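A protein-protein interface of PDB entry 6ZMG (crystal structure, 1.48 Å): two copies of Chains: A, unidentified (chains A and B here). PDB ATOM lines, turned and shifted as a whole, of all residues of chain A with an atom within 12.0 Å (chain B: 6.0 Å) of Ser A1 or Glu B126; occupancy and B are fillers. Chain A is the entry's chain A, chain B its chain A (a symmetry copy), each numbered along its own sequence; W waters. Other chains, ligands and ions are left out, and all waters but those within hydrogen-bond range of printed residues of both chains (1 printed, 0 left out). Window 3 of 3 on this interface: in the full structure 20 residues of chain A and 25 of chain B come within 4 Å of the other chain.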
ATOM      1  N   SER A   1      -2.786 -21.402  -9.839  1.00  0.00           N
ATOM      2  CA  SER A   1      -3.119 -22.852  -9.980  1.00  0.00           C
ATOM      3  C   SER A   1      -3.971 -23.291  -8.809  1.00  0.00           C
ATOM      4  O   SER A   1      -3.988 -22.640  -7.769  1.00  0.00           O
ATOM      5  CB  SER A   1      -1.847 -23.682 -10.057  1.00  0.00           C
ATOM      6  OG  SER A   1      -1.063 -23.497  -8.888  1.00  0.00           O
ATOM      7  N   LEU A   2      -4.698 -24.381  -9.002  1.00  0.00           N
ATOM      8  CA  LEU A   2      -5.594 -24.910  -7.995  1.00  0.00           C
ATOM      9  C   LEU A   2      -4.964 -26.128  -7.351  1.00  0.00           C
ATOM     10  O   LEU A   2      -4.486 -27.027  -8.046  1.00  0.00           O
ATOM     11  CB  LEU A   2      -6.895 -25.347  -8.640  1.00  0.00           C
ATOM     12  CG  LEU A   2      -7.829 -24.266  -9.143  1.00  0.00           C
ATOM     13  CD1 LEU A   2      -8.994 -24.981  -9.808  1.00  0.00           C
ATOM     14  CD2 LEU A   2      -8.288 -23.398  -8.012  1.00  0.00           C
ATOM     15  N   MET A   3      -5.078 -26.199  -6.020  1.00  0.00           N
ATOM     16  CA  MET A   3      -4.468 -27.246  -5.194  1.00  0.00           C
ATOM     17  C   MET A   3      -5.537 -28.288  -4.872  1.00  0.00           C
ATOM     18  O   MET A   3      -6.085 -28.337  -3.770  1.00  0.00           O
ATOM     19  CB  MET A   3      -3.925 -26.594  -3.917  1.00  0.00           C
ATOM     20  CG  MET A   3      -3.176 -27.496  -2.931  1.00  0.00           C
ATOM     21  SD  MET A   3      -1.524 -28.022  -3.440  1.00  0.00           S
ATOM     22  CE  MET A   3      -1.013 -26.598  -4.390  1.00  0.00           C
ATOM     23  N   GLU A   4      -5.818 -29.156  -5.847  1.00  0.00           N
ATOM     24  CA  GLU A   4      -6.959 -30.064  -5.771  1.00  0.00           C
ATOM     25  C   GLU A   4      -6.595 -31.270  -4.914  1.00  0.00           C
ATOM     26  O   GLU A   4      -5.741 -32.071  -5.299  1.00  0.00           O
ATOM     27  CB  GLU A   4      -7.328 -30.495  -7.194  1.00  0.00           C
ATOM     28  CG  GLU A   4      -7.659 -29.293  -8.121  1.00  0.00           C
ATOM     29  CD  GLU A   4      -8.092 -29.698  -9.524  1.00  0.00           C
ATOM     30  OE1 GLU A   4      -8.402 -28.803 -10.338  1.00  0.00           O
ATOM     31  OE2 GLU A   4      -8.122 -30.907  -9.822  1.00  0.00           O
ATOM     32  N   ARG A   5      -7.247 -31.417  -3.759  1.00  0.00           N
ATOM     33  CA  ARG A   5      -6.976 -32.553  -2.888  1.00  0.00           C
ATOM     34  C   ARG A   5      -7.675 -33.784  -3.443  1.00  0.00           C
ATOM     35  O   ARG A   5      -8.873 -33.742  -3.750  1.00  0.00           O
ATOM     36  CB  ARG A   5      -7.481 -32.307  -1.468  1.00  0.00           C
ATOM     37  CG  ARG A   5      -6.411 -31.882  -0.487  1.00  0.00           C
ATOM     38  CD  ARG A   5      -6.930 -31.828   0.953  1.00  0.00           C
ATOM     39  NE  ARG A   5      -5.932 -31.298   1.886  1.00  0.00           N
ATOM     40  CZ  ARG A   5      -5.509 -30.033   1.907  1.00  0.00           C
ATOM     41  NH1 ARG A   5      -5.981 -29.152   1.030  1.00  0.00           N
ATOM     42  NH2 ARG A   5      -4.597 -29.656   2.796  1.00  0.00           N
ATOM     43  N   ARG B  62      -8.589 -31.471 -20.580  1.00  0.00           N
ATOM     44  CA  ARG B  62      -9.520 -30.666 -21.370  1.00  0.00           C
ATOM     45  C   ARG B  62      -9.999 -31.396 -22.620  1.00  0.00           C
ATOM     46  O   ARG B  62     -11.180 -31.315 -22.980  1.00  0.00           O
ATOM     47  CB  ARG B  62      -8.844 -29.332 -21.712  1.00  0.00           C
ATOM     48  CG  ARG B  62      -8.630 -28.432 -20.474  1.00  0.00           C
ATOM     49  CD  ARG B  62      -7.435 -27.473 -20.583  1.00  0.00           C
ATOM     50  NE  ARG B  62      -7.298 -26.645 -19.379  1.00  0.00           N
ATOM     51  CZ  ARG B  62      -6.726 -27.050 -18.245  1.00  0.00           C
ATOM     52  NH1 ARG B  62      -6.237 -28.276 -18.152  1.00  0.00           N
ATOM     53  NH2 ARG B  62      -6.649 -26.236 -17.201  1.00  0.00           N
ATOM     54  N   LYS B  96       4.069 -26.091  -6.984  1.00  0.00           N
ATOM     55  CA  LYS B  96       3.407 -25.030  -7.733  1.00  0.00           C
ATOM     56  C   LYS B  96       4.380 -24.351  -8.682  1.00  0.00           C
ATOM     57  O   LYS B  96       4.031 -24.042  -9.828  1.00  0.00           O
ATOM     58  CB  LYS B  96       2.799 -24.014  -6.772  1.00  0.00           C
ATOM     59  CG  LYS B  96       1.505 -24.455  -6.146  1.00  0.00           C
ATOM     60  CD  LYS B  96       0.892 -23.285  -5.379  1.00  0.00           C
ATOM     61  CE  LYS B  96      -0.614 -23.504  -5.155  1.00  0.00           C
ATOM     62  NZ  LYS B  96      -1.471 -22.398  -5.699  1.00  0.00           N
ATOM     63  N   ARG B  99       5.246 -26.610 -11.655  1.00  0.00           N
ATOM     64  CA  ARG B  99       4.185 -26.633 -12.653  1.00  0.00           C
ATOM     65  C   ARG B  99       4.320 -25.461 -13.612  1.00  0.00           C
ATOM     66  O   ARG B  99       4.180 -25.621 -14.830  1.00  0.00           O
ATOM     67  CB  ARG B  99       2.810 -26.597 -11.991  1.00  0.00           C
ATOM     68  CG  ARG B  99       1.697 -26.855 -12.997  1.00  0.00           C
ATOM     69  CD  ARG B  99       0.455 -25.989 -12.828  1.00  0.00           C
ATOM     70  NE  ARG B  99       0.746 -24.561 -12.785  1.00  0.00           N
ATOM     71  CZ  ARG B  99       1.010 -23.798 -13.841  1.00  0.00           C
ATOM     72  NH1 ARG B  99       1.001 -24.299 -15.072  1.00  0.00           N
ATOM     73  NH2 ARG B  99       1.253 -22.505 -13.652  1.00  0.00           N
ATOM     74  N   ILE B 123      -1.867 -30.316  -8.569  1.00  0.00           N
ATOM     75  CA  ILE B 123      -1.724 -28.879  -8.732  1.00  0.00           C
ATOM     76  C   ILE B 123      -2.031 -28.606 -10.192  1.00  0.00           C
ATOM     77  O   ILE B 123      -1.272 -29.028 -11.065  1.00  0.00           O
ATOM     78  CB  ILE B 123      -0.314 -28.420  -8.374  1.00  0.00           C
ATOM     79  CG1 ILE B 123      -0.009 -28.758  -6.920  1.00  0.00           C
ATOM     80  CG2 ILE B 123      -0.207 -26.935  -8.612  1.00  0.00           C
ATOM     81  CD1 ILE B 123       1.424 -28.495  -6.506  1.00  0.00           C
ATOM     82  N   THR B 124      -3.136 -27.914 -10.456  1.00  0.00           N
ATOM     83  CA  THR B 124      -3.724 -27.851 -11.785  1.00  0.00           C
ATOM     84  C   THR B 124      -3.728 -26.429 -12.311  1.00  0.00           C
ATOM     85  O   THR B 124      -4.156 -25.503 -11.617  1.00  0.00           O
ATOM     86  CB  THR B 124      -5.148 -28.394 -11.739  1.00  0.00           C
ATOM     87  OG1 THR B 124      -5.101 -29.709 -11.187  1.00  0.00           O
ATOM     88  CG2 THR B 124      -5.709 -28.475 -13.102  1.00  0.00           C
ATOM     89  N   ALA B 125      -3.273 -26.277 -13.547  1.00  0.00           N
ATOM     90  CA  ALA B 125      -3.267 -24.976 -14.187  1.00  0.00           C
ATOM     91  C   ALA B 125      -4.690 -24.475 -14.369  1.00  0.00           C
ATOM     92  O   ALA B 125      -5.607 -25.237 -14.696  1.00  0.00           O
ATOM     93  CB  ALA B 125      -2.610 -25.093 -15.558  1.00  0.00           C
ATOM     94  N   GLU B 126      -4.855 -23.169 -14.200  1.00  0.00           N
ATOM     95  CA  GLU B 126      -6.132 -22.492 -14.369  1.00  0.00           C
ATOM     96  C   GLU B 126      -6.226 -21.768 -15.707  1.00  0.00           C
ATOM     97  O   GLU B 126      -6.894 -20.731 -15.825  1.00  0.00           O
ATOM     98  CB  GLU B 126      -6.353 -21.555 -13.189  1.00  0.00           C
ATOM     99  CG  GLU B 126      -6.515 -22.291 -11.866  1.00  0.00           C
ATOM    100  CD  GLU B 126      -6.687 -21.334 -10.706  1.00  0.00           C
ATOM    101  OE1 GLU B 126      -7.670 -20.585 -10.692  1.00  0.00           O
ATOM    102  OE2 GLU B 126      -5.841 -21.303  -9.809  1.00  0.00           O
ATOM    103  N   TRP B 127      -5.559 -22.304 -16.728  1.00  0.00           N
ATOM    104  CA  TRP B 127      -5.627 -21.738 -18.066  1.00  0.00           C
ATOM    105  C   TRP B 127      -7.072 -21.470 -18.469  1.00  0.00           C
ATOM    106  O   TRP B 127      -7.943 -22.349 -18.370  1.00  0.00           O
ATOM    107  CB  TRP B 127      -4.996 -22.719 -19.052  1.00  0.00           C
ATOM    108  CG  TRP B 127      -3.563 -23.052 -18.780  1.00  0.00           C
ATOM    109  CD1 TRP B 127      -2.609 -22.249 -18.206  1.00  0.00           C
ATOM    110  CD2 TRP B 127      -2.910 -24.289 -19.081  1.00  0.00           C
ATOM    111  NE1 TRP B 127      -1.404 -22.917 -18.142  1.00  0.00           N
ATOM    112  CE2 TRP B 127      -1.571 -24.174 -18.661  1.00  0.00           C
ATOM    113  CE3 TRP B 127      -3.329 -25.483 -19.672  1.00  0.00           C
ATOM    114  CZ2 TRP B 127      -0.654 -25.199 -18.828  1.00  0.00           C
ATOM    115  CZ3 TRP B 127      -2.420 -26.498 -19.827  1.00  0.00           C
ATOM    116  CH2 TRP B 127      -1.101 -26.355 -19.405  1.00  0.00           C
ATOM    117  N   TYR B 128      -7.309 -20.253 -18.954  1.00  0.00           N
ATOM    118  CA  TYR B 128      -8.660 -19.816 -19.255  1.00  0.00           C
ATOM    119  C   TYR B 128      -9.274 -20.664 -20.362  1.00  0.00           C
ATOM    120  O   TYR B 128      -8.633 -20.939 -21.380  1.00  0.00           O
ATOM    121  CB  TYR B 128      -8.654 -18.344 -19.672  1.00  0.00           C
ATOM    122  CG  TYR B 128     -10.058 -17.825 -19.787  1.00  0.00           C
ATOM    123  CD1 TYR B 128     -10.741 -17.424 -18.666  1.00  0.00           C
ATOM    124  CD2 TYR B 128     -10.725 -17.814 -20.992  1.00  0.00           C
ATOM    125  CE1 TYR B 128     -12.023 -16.995 -18.730  1.00  0.00           C
ATOM    126  CE2 TYR B 128     -12.039 -17.371 -21.068  1.00  0.00           C
ATOM    127  CZ  TYR B 128     -12.677 -16.967 -19.927  1.00  0.00           C
ATOM    128  OH  TYR B 128     -13.985 -16.549 -19.963  1.00  0.00           O
ATOM    129  N   GLU B 129     -10.529 -21.063 -20.169  1.00  0.00           N
ATOM    130  CA  GLU B 129     -11.237 -21.830 -21.190  1.00  0.00           C
ATOM    131  C   GLU B 129     -12.479 -21.097 -21.683  1.00  0.00           C
ATOM    132  O   GLU B 129     -13.415 -20.882 -20.918  1.00  0.00           O
ATOM    133  CB  GLU B 129     -11.619 -23.214 -20.661  1.00  0.00           C
HETATM  134  O   HOH W   1      -1.265 -20.327  -7.640  1.00  0.00           O
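NZ of Lys B96 lies within hydrogen-bond range of O of Ser A1, 3.3 Å away.
N of Leu A2 sits at hydrogen-bond distance from OE2 of Glu B126 (3.4 Å).
The side-chain carboxylate (OE2) of Glu B126 lies close to the backbone NH (N) of Ser A1, 3.1 Å away.
The backbone NH (N) of Leu A2 is in hydrogen-bond range of the backbone carbonyl oxygen (O) of Thr B124, 2.9 Å away.
Among the printed residues, merely in contact across the chains: Met A3 with Lys B96 (3.2 Å), Ser A1 with Thr B124 (3.3 Å), Leu A2 with Ile B123 (3.4 Å), Glu A4 with Thr B124 (3.4 Å), Met A3 with Ile B123 (3.5 Å), Ser A1 with Ile B123 (3.6 Å) and Ser A1 with Arg B99 (3.9 Å).
Of the printed residues of chain B, Leu A2 touches Ile B123 (3.4 Å), Thr B124 (2.9 Å) and Glu B126 (3.4 Å).
Of the printed residues of chain B, Met A3 touches Lys B96 and Ile B123.
Of the printed residues of chain B, Glu A4 touches Thr B124.
Arg A5 touches none of the printed residues of chain B.
Of chain A, only Ser A1 (3.9 Å) comes within 4 Å of Arg B99.
Printed residues of chain A within 4 Å of Ile B123: Ser A1, Leu A2 and Met A3.
Of chain A, only Ser A1 (2.9 Å) and Leu A2 (3.4 Å) come within 4 Å of Glu B126.
No residue of chain A comes within 4 Å of Trp B127.
The nearest printed residue of chain A that does not touch Glu B126 is Met A3 (6.2 Å).
The nearest printed residue of chain B that does not touch Leu A2 is Lys B96 (5.0 Å).
Hydrophobic or aromatic side chains of chain B within 4 Å of the printed part of chain A: Ile B123.
Hydrophobic or aromatic side chains of chain A that line the printed part of chain B: Leu A2 and Met A3.
Among the printed residues, 11 pairs touch across the chains.
Among the printed residues, no Asp or Glu carboxylate lies within 4 Å of a Lys or Arg side-chain nitrogen of the other chain.
No position is printed for both chains.
Water W1 bridges NZ of Lys B96 and N of Ser A1.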
